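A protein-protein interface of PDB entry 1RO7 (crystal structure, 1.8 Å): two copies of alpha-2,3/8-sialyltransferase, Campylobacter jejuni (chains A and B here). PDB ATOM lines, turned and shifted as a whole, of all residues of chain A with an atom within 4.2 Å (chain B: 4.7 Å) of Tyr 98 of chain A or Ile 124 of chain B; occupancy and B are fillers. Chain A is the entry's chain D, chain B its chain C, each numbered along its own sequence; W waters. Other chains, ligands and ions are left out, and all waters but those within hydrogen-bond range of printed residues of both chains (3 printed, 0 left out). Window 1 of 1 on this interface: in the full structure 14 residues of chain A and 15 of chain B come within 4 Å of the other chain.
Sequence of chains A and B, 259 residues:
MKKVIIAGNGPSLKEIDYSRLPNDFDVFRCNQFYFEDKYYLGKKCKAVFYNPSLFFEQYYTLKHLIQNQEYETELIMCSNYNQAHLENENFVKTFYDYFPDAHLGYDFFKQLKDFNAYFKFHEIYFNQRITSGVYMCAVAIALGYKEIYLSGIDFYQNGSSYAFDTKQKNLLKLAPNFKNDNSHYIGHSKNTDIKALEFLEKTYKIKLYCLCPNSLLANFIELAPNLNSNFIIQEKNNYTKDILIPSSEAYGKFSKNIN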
ATOM      1  N   PHE A  56     -33.000  16.877   1.559  1.00  0.00           N
ATOM      2  CA  PHE A  56     -31.983  17.805   1.076  1.00  0.00           C
ATOM      3  C   PHE A  56     -31.600  18.795   2.170  1.00  0.00           C
ATOM      4  O   PHE A  56     -30.414  18.989   2.459  1.00  0.00           O
ATOM      5  CB  PHE A  56     -32.505  18.555  -0.156  1.00  0.00           C
ATOM      6  CG  PHE A  56     -31.525  19.543  -0.731  1.00  0.00           C
ATOM      7  CD1 PHE A  56     -30.287  19.124  -1.204  1.00  0.00           C
ATOM      8  CD2 PHE A  56     -31.852  20.894  -0.811  1.00  0.00           C
ATOM      9  CE1 PHE A  56     -29.387  20.038  -1.755  1.00  0.00           C
ATOM     10  CE2 PHE A  56     -30.961  21.816  -1.357  1.00  0.00           C
ATOM     11  CZ  PHE A  56     -29.725  21.385  -1.832  1.00  0.00           C
ATOM     12  N   THR A  94     -30.627   8.592  -7.945  1.00  0.00           N
ATOM     13  CA  THR A  94     -29.276   9.131  -7.794  1.00  0.00           C
ATOM     14  C   THR A  94     -28.821   9.305  -6.352  1.00  0.00           C
ATOM     15  O   THR A  94     -27.718   9.783  -6.102  1.00  0.00           O
ATOM     16  CB  THR A  94     -29.181  10.499  -8.472  1.00  0.00           C
ATOM     17  OG1 THR A  94     -30.080  11.408  -7.822  1.00  0.00           O
ATOM     18  CG2 THR A  94     -29.567  10.395  -9.946  1.00  0.00           C
ATOM     19  N   PHE A  95     -29.668   8.904  -5.413  1.00  0.00           N
ATOM     20  CA  PHE A  95     -29.386   9.064  -3.992  1.00  0.00           C
ATOM     21  C   PHE A  95     -27.962   8.833  -3.503  1.00  0.00           C
ATOM     22  O   PHE A  95     -27.365   9.718  -2.887  1.00  0.00           O
ATOM     23  CB  PHE A  95     -30.337   8.188  -3.171  1.00  0.00           C
ATOM     24  CG  PHE A  95     -30.244   8.429  -1.693  1.00  0.00           C
ATOM     25  CD1 PHE A  95     -29.410   7.650  -0.896  1.00  0.00           C
ATOM     26  CD2 PHE A  95     -30.990   9.445  -1.098  1.00  0.00           C
ATOM     27  CE1 PHE A  95     -29.321   7.877   0.474  1.00  0.00           C
ATOM     28  CE2 PHE A  95     -30.910   9.683   0.271  1.00  0.00           C
ATOM     29  CZ  PHE A  95     -30.074   8.895   1.059  1.00  0.00           C
ATOM     30  N   TYR A  96     -27.419   7.649  -3.752  1.00  0.00           N
ATOM     31  CA  TYR A  96     -26.075   7.347  -3.282  1.00  0.00           C
ATOM     32  C   TYR A  96     -24.971   8.193  -3.897  1.00  0.00           C
ATOM     33  O   TYR A  96     -23.868   8.265  -3.352  1.00  0.00           O
ATOM     34  CB  TYR A  96     -25.769   5.862  -3.477  1.00  0.00           C
ATOM     35  CG  TYR A  96     -26.591   4.999  -2.554  1.00  0.00           C
ATOM     36  CD1 TYR A  96     -27.746   4.360  -3.006  1.00  0.00           C
ATOM     37  CD2 TYR A  96     -26.244   4.871  -1.211  1.00  0.00           C
ATOM     38  CE1 TYR A  96     -28.538   3.611  -2.131  1.00  0.00           C
ATOM     39  CE2 TYR A  96     -27.024   4.134  -0.334  1.00  0.00           C
ATOM     40  CZ  TYR A  96     -28.170   3.508  -0.798  1.00  0.00           C
ATOM     41  OH  TYR A  96     -28.959   2.808   0.085  1.00  0.00           O
ATOM     42  N   ASP A  97     -25.250   8.828  -5.025  1.00  0.00           N
ATOM     43  CA  ASP A  97     -24.229   9.663  -5.636  1.00  0.00           C
ATOM     44  C   ASP A  97     -24.257  11.090  -5.091  1.00  0.00           C
ATOM     45  O   ASP A  97     -23.248  11.789  -5.133  1.00  0.00           O
ATOM     46  CB  ASP A  97     -24.353   9.635  -7.163  1.00  0.00           C
ATOM     47  CG  ASP A  97     -23.978   8.277  -7.743  1.00  0.00           C
ATOM     48  OD1 ASP A  97     -23.078   7.618  -7.177  1.00  0.00           O
ATOM     49  OD2 ASP A  97     -24.568   7.867  -8.758  1.00  0.00           O
ATOM     50  N   TYR A  98     -25.403  11.520  -4.565  1.00  0.00           N
ATOM     51  CA  TYR A  98     -25.507  12.849  -3.972  1.00  0.00           C
ATOM     52  C   TYR A  98     -25.221  12.788  -2.470  1.00  0.00           C
ATOM     53  O   TYR A  98     -24.735  13.754  -1.885  1.00  0.00           O
ATOM     54  CB  TYR A  98     -26.903  13.456  -4.191  1.00  0.00           C
ATOM     55  CG  TYR A  98     -27.121  13.997  -5.582  1.00  0.00           C
ATOM     56  CD1 TYR A  98     -27.491  13.156  -6.628  1.00  0.00           C
ATOM     57  CD2 TYR A  98     -26.916  15.350  -5.861  1.00  0.00           C
ATOM     58  CE1 TYR A  98     -27.655  13.651  -7.925  1.00  0.00           C
ATOM     59  CE2 TYR A  98     -27.072  15.853  -7.150  1.00  0.00           C
ATOM     60  CZ  TYR A  98     -27.441  14.999  -8.175  1.00  0.00           C
ATOM     61  OH  TYR A  98     -27.597  15.488  -9.451  1.00  0.00           O
ATOM     62  N   PHE A  99     -25.498  11.639  -1.860  1.00  0.00           N
ATOM     63  CA  PHE A  99     -25.293  11.451  -0.420  1.00  0.00           C
ATOM     64  C   PHE A  99     -24.591  10.117  -0.189  1.00  0.00           C
ATOM     65  O   PHE A  99     -25.177   9.171   0.341  1.00  0.00           O
ATOM     66  CB  PHE A  99     -26.650  11.443   0.280  1.00  0.00           C
ATOM     67  CG  PHE A  99     -27.523  12.609  -0.092  1.00  0.00           C
ATOM     68  CD1 PHE A  99     -27.258  13.878   0.409  1.00  0.00           C
ATOM     69  CD2 PHE A  99     -28.602  12.437  -0.954  1.00  0.00           C
ATOM     70  CE1 PHE A  99     -28.052  14.965   0.058  1.00  0.00           C
ATOM     71  CE2 PHE A  99     -29.406  13.517  -1.313  1.00  0.00           C
ATOM     72  CZ  PHE A  99     -29.131  14.783  -0.807  1.00  0.00           C
ATOM     73  N   PRO A 100     -23.308  10.034  -0.561  1.00  0.00           N
ATOM     74  CA  PRO A 100     -22.509   8.815  -0.421  1.00  0.00           C
ATOM     75  C   PRO A 100     -22.474   8.106   0.919  1.00  0.00           C
ATOM     76  O   PRO A 100     -22.271   6.893   0.957  1.00  0.00           O
ATOM     77  CB  PRO A 100     -21.114   9.265  -0.852  1.00  0.00           C
ATOM     78  CG  PRO A 100     -21.401  10.371  -1.811  1.00  0.00           C
ATOM     79  CD  PRO A 100     -22.492  11.127  -1.112  1.00  0.00           C
ATOM     80  N   ALA A 250     -27.221  25.859  -4.313  1.00  0.00           N
ATOM     81  CA  ALA A 250     -27.334  24.465  -3.905  1.00  0.00           C
ATOM     82  C   ALA A 250     -28.640  23.901  -4.453  1.00  0.00           C
ATOM     83  O   ALA A 250     -28.661  22.820  -5.036  1.00  0.00           O
ATOM     84  CB  ALA A 250     -27.316  24.367  -2.393  1.00  0.00           C
ATOM     85  N   LYS A 253     -28.734  23.021  -8.073  1.00  0.00           N
ATOM     86  CA  LYS A 253     -28.041  21.779  -8.386  1.00  0.00           C
ATOM     87  C   LYS A 253     -28.859  20.528  -8.073  1.00  0.00           C
ATOM     88  O   LYS A 253     -28.708  19.500  -8.730  1.00  0.00           O
ATOM     89  CB  LYS A 253     -26.720  21.728  -7.621  1.00  0.00           C
ATOM     90  CG  LYS A 253     -25.731  22.806  -8.025  1.00  0.00           C
ATOM     91  CD  LYS A 253     -24.452  22.720  -7.214  1.00  0.00           C
ATOM     92  CE  LYS A 253     -23.455  23.789  -7.658  1.00  0.00           C
ATOM     93  NZ  LYS A 253     -22.216  23.813  -6.826  1.00  0.00           N
ATOM     94  N   PHE A 254     -29.732  20.625  -7.075  1.00  0.00           N
ATOM     95  CA  PHE A 254     -30.553  19.496  -6.645  1.00  0.00           C
ATOM     96  C   PHE A 254     -32.001  19.615  -7.120  1.00  0.00           C
ATOM     97  O   PHE A 254     -32.834  18.751  -6.831  1.00  0.00           O
ATOM     98  CB  PHE A 254     -30.506  19.413  -5.113  1.00  0.00           C
ATOM     99  CG  PHE A 254     -30.886  18.069  -4.552  1.00  0.00           C
ATOM    100  CD1 PHE A 254     -32.139  17.863  -3.980  1.00  0.00           C
ATOM    101  CD2 PHE A 254     -29.974  17.020  -4.564  1.00  0.00           C
ATOM    102  CE1 PHE A 254     -32.479  16.625  -3.422  1.00  0.00           C
ATOM    103  CE2 PHE A 254     -30.298  15.781  -4.011  1.00  0.00           C
ATOM    104  CZ  PHE A 254     -31.554  15.584  -3.437  1.00  0.00           C
ATOM    105  N   ASN A 257     -34.214  16.769  -8.321  1.00  0.00           N
ATOM    106  CA  ASN A 257     -34.583  15.741  -7.356  1.00  0.00           C
ATOM    107  C   ASN A 257     -35.613  16.206  -6.333  1.00  0.00           C
ATOM    108  O   ASN A 257     -35.891  15.498  -5.362  1.00  0.00           O
ATOM    109  CB  ASN A 257     -33.336  15.226  -6.632  1.00  0.00           C
ATOM    110  CG  ASN A 257     -32.286  14.693  -7.590  1.00  0.00           C
ATOM    111  OD1 ASN A 257     -32.617  14.132  -8.633  1.00  0.00           O
ATOM    112  ND2 ASN A 257     -31.015  14.853  -7.234  1.00  0.00           N
ATOM    113  N   GLN B  83     -22.553  13.248 -11.263  1.00  0.00           N
ATOM    114  CA  GLN B  83     -23.352  14.412 -10.885  1.00  0.00           C
ATOM    115  C   GLN B  83     -23.828  15.076 -12.171  1.00  0.00           C
ATOM    116  O   GLN B  83     -23.014  15.475 -13.007  1.00  0.00           O
ATOM    117  CB  GLN B  83     -22.506  15.400 -10.083  1.00  0.00           C
ATOM    118  CG  GLN B  83     -22.131  14.934  -8.691  1.00  0.00           C
ATOM    119  CD  GLN B  83     -23.316  14.923  -7.751  1.00  0.00           C
ATOM    120  OE1 GLN B  83     -24.154  14.018  -7.789  1.00  0.00           O
ATOM    121  NE2 GLN B  83     -23.403  15.939  -6.907  1.00  0.00           N
ATOM    122  N   ALA B  84     -25.143  15.201 -12.323  1.00  0.00           N
ATOM    123  CA  ALA B  84     -25.721  15.791 -13.527  1.00  0.00           C
ATOM    124  C   ALA B  84     -25.234  17.202 -13.840  1.00  0.00           C
ATOM    125  O   ALA B  84     -25.168  17.588 -15.006  1.00  0.00           O
ATOM    126  CB  ALA B  84     -27.252  15.776 -13.437  1.00  0.00           C
ATOM    127  N   HIS B  85     -24.894  17.978 -12.818  1.00  0.00           N
ATOM    128  CA  HIS B  85     -24.437  19.341 -13.071  1.00  0.00           C
ATOM    129  C   HIS B  85     -22.943  19.439 -13.339  1.00  0.00           C
ATOM    130  O   HIS B  85     -22.435  20.515 -13.666  1.00  0.00           O
ATOM    131  CB  HIS B  85     -24.810  20.266 -11.908  1.00  0.00           C
ATOM    132  CG  HIS B  85     -24.243  19.846 -10.588  1.00  0.00           C
ATOM    133  ND1 HIS B  85     -24.689  18.732  -9.909  1.00  0.00           N
ATOM    134  CD2 HIS B  85     -23.262  20.385  -9.827  1.00  0.00           C
ATOM    135  CE1 HIS B  85     -24.005  18.605  -8.786  1.00  0.00           C
ATOM    136  NE2 HIS B  85     -23.134  19.594  -8.713  1.00  0.00           N
ATOM    137  N   LYS B 120     -18.842  15.636  -2.199  1.00  0.00           N
ATOM    138  CA  LYS B 120     -20.209  15.950  -2.594  1.00  0.00           C
ATOM    139  C   LYS B 120     -20.862  17.011  -1.710  1.00  0.00           C
ATOM    140  O   LYS B 120     -21.507  17.936  -2.210  1.00  0.00           O
ATOM    141  CB  LYS B 120     -21.056  14.669  -2.606  1.00  0.00           C
ATOM    142  CG  LYS B 120     -20.594  13.622  -3.631  1.00  0.00           C
ATOM    143  CD  LYS B 120     -20.852  14.088  -5.065  1.00  0.00           C
ATOM    144  CE  LYS B 120     -20.217  13.160  -6.102  1.00  0.00           C
ATOM    145  NZ  LYS B 120     -20.666  11.735  -6.014  1.00  0.00           N
ATOM    146  N   PHE B 121     -20.698  16.893  -0.398  1.00  0.00           N
ATOM    147  CA  PHE B 121     -21.306  17.870   0.492  1.00  0.00           C
ATOM    148  C   PHE B 121     -20.816  19.293   0.237  1.00  0.00           C
ATOM    149  O   PHE B 121     -21.615  20.228   0.146  1.00  0.00           O
ATOM    150  CB  PHE B 121     -21.056  17.506   1.956  1.00  0.00           C
ATOM    151  CG  PHE B 121     -21.610  18.512   2.919  1.00  0.00           C
ATOM    152  CD1 PHE B 121     -20.767  19.325   3.660  1.00  0.00           C
ATOM    153  CD2 PHE B 121     -22.987  18.676   3.048  1.00  0.00           C
ATOM    154  CE1 PHE B 121     -21.281  20.294   4.520  1.00  0.00           C
ATOM    155  CE2 PHE B 121     -23.518  19.647   3.904  1.00  0.00           C
ATOM    156  CZ  PHE B 121     -22.661  20.458   4.641  1.00  0.00           C
ATOM    157  N   HIS B 122     -19.506  19.465   0.115  1.00  0.00           N
ATOM    158  CA  HIS B 122     -18.958  20.798  -0.121  1.00  0.00           C
ATOM    159  C   HIS B 122     -19.239  21.353  -1.506  1.00  0.00           C
ATOM    160  O   HIS B 122     -19.386  22.565  -1.671  1.00  0.00           O
ATOM    161  CB  HIS B 122     -17.453  20.810   0.156  1.00  0.00           C
ATOM    162  CG  HIS B 122     -17.118  20.597   1.597  1.00  0.00           C
ATOM    163  ND1 HIS B 122     -17.077  19.347   2.174  1.00  0.00           N
ATOM    164  CD2 HIS B 122     -16.900  21.482   2.599  1.00  0.00           C
ATOM    165  CE1 HIS B 122     -16.855  19.470   3.470  1.00  0.00           C
ATOM    166  NE2 HIS B 122     -16.744  20.755   3.754  1.00  0.00           N
ATOM    167  N   GLU B 123     -19.324  20.485  -2.504  1.00  0.00           N
ATOM    168  CA  GLU B 123     -19.591  20.953  -3.856  1.00  0.00           C
ATOM    169  C   GLU B 123     -21.064  21.299  -4.010  1.00  0.00           C
ATOM    170  O   GLU B 123     -21.407  22.367  -4.513  1.00  0.00           O
ATOM    171  CB  GLU B 123     -19.186  19.894  -4.889  1.00  0.00           C
ATOM    172  CG  GLU B 123     -19.106  20.434  -6.316  1.00  0.00           C
ATOM    173  CD  GLU B 123     -20.468  20.698  -6.922  1.00  0.00           C
ATOM    174  OE1 GLU B 123     -20.588  21.630  -7.748  1.00  0.00           O
ATOM    175  OE2 GLU B 123     -21.419  19.964  -6.581  1.00  0.00           O
ATOM    176  N   ILE B 124     -21.934  20.399  -3.562  1.00  0.00           N
ATOM    177  CA  ILE B 124     -23.374  20.615  -3.668  1.00  0.00           C
ATOM    178  C   ILE B 124     -23.873  21.810  -2.861  1.00  0.00           C
ATOM    179  O   ILE B 124     -24.557  22.695  -3.385  1.00  0.00           O
ATOM    180  CB  ILE B 124     -24.158  19.360  -3.203  1.00  0.00           C
ATOM    181  CG1 ILE B 124     -23.942  18.213  -4.194  1.00  0.00           C
ATOM    182  CG2 ILE B 124     -25.634  19.689  -3.055  1.00  0.00           C
ATOM    183  CD1 ILE B 124     -24.435  16.866  -3.687  1.00  0.00           C
ATOM    184  N   TYR B 125     -23.526  21.836  -1.583  1.00  0.00           N
ATOM    185  CA  TYR B 125     -23.997  22.892  -0.708  1.00  0.00           C
ATOM    186  C   TYR B 125     -23.139  24.152  -0.594  1.00  0.00           C
ATOM    187  O   TYR B 125     -23.660  25.225  -0.284  1.00  0.00           O
ATOM    188  CB  TYR B 125     -24.238  22.318   0.686  1.00  0.00           C
ATOM    189  CG  TYR B 125     -25.283  21.227   0.727  1.00  0.00           C
ATOM    190  CD1 TYR B 125     -24.934  19.884   0.563  1.00  0.00           C
ATOM    191  CD2 TYR B 125     -26.628  21.537   0.947  1.00  0.00           C
ATOM    192  CE1 TYR B 125     -25.905  18.873   0.628  1.00  0.00           C
ATOM    193  CE2 TYR B 125     -27.599  20.541   1.010  1.00  0.00           C
ATOM    194  CZ  TYR B 125     -27.235  19.215   0.858  1.00  0.00           C
ATOM    195  OH  TYR B 125     -28.197  18.232   0.977  1.00  0.00           O
ATOM    196  N   PHE B 126     -21.838  24.043  -0.839  1.00  0.00           N
ATOM    197  CA  PHE B 126     -20.986  25.222  -0.711  1.00  0.00           C
ATOM    198  C   PHE B 126     -20.250  25.636  -1.973  1.00  0.00           C
ATOM    199  O   PHE B 126     -19.460  26.588  -1.958  1.00  0.00           O
ATOM    200  CB  PHE B 126     -19.999  25.020   0.435  1.00  0.00           C
ATOM    201  CG  PHE B 126     -20.656  24.936   1.777  1.00  0.00           C
ATOM    202  CD1 PHE B 126     -20.633  23.755   2.504  1.00  0.00           C
ATOM    203  CD2 PHE B 126     -21.330  26.033   2.303  1.00  0.00           C
ATOM    204  CE1 PHE B 126     -21.274  23.663   3.735  1.00  0.00           C
ATOM    205  CE2 PHE B 126     -21.977  25.950   3.535  1.00  0.00           C
ATOM    206  CZ  PHE B 126     -21.947  24.762   4.250  1.00  0.00           C
ATOM    207  N   ASN B 127     -20.514  24.920  -3.059  1.00  0.00           N
ATOM    208  CA  ASN B 127     -19.908  25.208  -4.351  1.00  0.00           C
ATOM    209  C   ASN B 127     -18.388  25.113  -4.334  1.00  0.00           C
ATOM    210  O   ASN B 127     -17.708  25.755  -5.135  1.00  0.00           O
ATOM    211  CB  ASN B 127     -20.340  26.593  -4.829  1.00  0.00           C
ATOM    212  CG  ASN B 127     -20.091  26.795  -6.301  1.00  0.00           C
ATOM    213  OD1 ASN B 127     -20.415  25.930  -7.118  1.00  0.00           O
ATOM    214  ND2 ASN B 127     -19.523  27.943  -6.656  1.00  0.00           N
HETATM  215  O   HOH W   1     -23.531  24.912  -4.438  1.00  0.00           O
HETATM  216  O   HOH W   2     -27.237  17.960 -10.163  1.00  0.00           O
HETATM  217  O   HOH W   3     -24.026  15.939  -0.058  1.00  0.00           O
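O of Asp 97 of chain A touches OE1 of Gln 83 of chain B, 3.6 Å away.
Tyr 98 of chain A touches Gln 83 of chain B.
Ala 84 of chain B touches Tyr 98 of chain A (N to OH, 3.8 Å).
O of Tyr 98 of chain A touches CB of Lys 120 of chain B, 3.9 Å away.
O of Tyr 98 of chain A touches CD1 of Ile 124 of chain B, at 3.6 Å.
Tyr 125 of chain B touches Phe 99 of chain A (OH to CE1, 3.4 Å).
Pro 100 of chain A touches Lys 120 of chain B (CG to CG, 3.8 Å).
Ala 250 of chain A touches Ile 124 of chain B (CA to O, 3.3 Å).
CD2 of His 85 of chain B touches CD of Lys 253 of chain A (3.7 Å).
Lys 253 of chain A touches Ile 124 of chain B (CD to O, 3.8 Å).
Hydrophobic or aromatic side chains of chain B within 4 Å of the printed part of chain A: His 85, Ile 124 and Tyr 125.
Of the 12 printed residues of chain A, 7 touch a printed residue of chain B.
Hydrophobic or aromatic side chains of chain A within 4 Å of the printed part of chain B: Phe 56, Tyr 98, Phe 99, Pro 100 and Ala 250.
Along chain A the printed residues that touch a printed residue of chain B span positions 56 to 253.
Among the printed residues, 15 pairs touch across the chains.
A ring nitrogen (NE2) of His 85 of chain B lies within hydrogen-bond range of the side-chain carboxylate of Glu 123 of chain B (2.8 Å).
O of His 122 of chain B sits at hydrogen-bond distance from N of Asn 127 of chain B.
NZ of Lys 120 of chain B is in hydrogen-bond range of O of Asp 97 of chain A (2.7 Å).
OD1 of Asn 127 of chain B sits at hydrogen-bond distance from NZ of Lys 253 of chain A.
The side-chain carboxylate of Glu 123 of chain B is in salt-bridge range of the side-chain amino group of Lys 253 of chain A.
The backbone carbonyl oxygen of Phe 56 of chain A lies within hydrogen-bond range of the side-chain hydroxyl of Tyr 125 of chain B (2.8 Å).
Thr 94 of chain A touches none of the printed residues of chain B.
Printed residues of chain B within 4 Å of Phe 99 of chain A: Tyr 125 (3.4 Å).
Of the printed residues of chain B, Pro 100 of chain A touches Lys 120.
Printed residues of chain B within 4 Å of Lys 253 of chain A: His 85, Glu 123, Ile 124 and Asn 127.
Of the printed residues of chain A, Gln 83 of chain B touches Asp 97 and Tyr 98.
Of the printed residues of chain A, Lys 120 of chain B touches Asp 97 (2.7 Å), Tyr 98 (3.9 Å) and Pro 100 (3.8 Å).
Printed residues of chain A within 4 Å of Ile 124 of chain B: Phe 56, Tyr 98, Ala 250 and Lys 253.
Phe 126 of chain B touches none of the printed residues of chain A.
The nearest printed residue of chain A that does not touch Ile 124 of chain B is Phe 254 of chain A (5.3 Å).
The nearest printed residue of chain B that does not touch Pro 100 of chain A is Phe 121 of chain B (6.1 Å).
Water W2 lies within hydrogen-bond range of O of Lys 253 of chain A (2.6 Å), OH of Tyr 98 of chain A (2.6 Å) and ND1 of His 85 of chain B (2.7 Å).
Water W1 lies within hydrogen-bond range of O of Ile 124 of chain B (2.7 Å), NZ of Lys 253 of chain A (2.9 Å), O of Glu 123 of chain B (3.3 Å) and N of Asn 127 of chain B (3.3 Å).
Water W3 bridges the backbone carbonyl oxygen of Tyr 98 of chain A (2.9 Å) and the backbone NH of Phe 121 of chain B (3.5 Å).
No position is printed for both chains.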
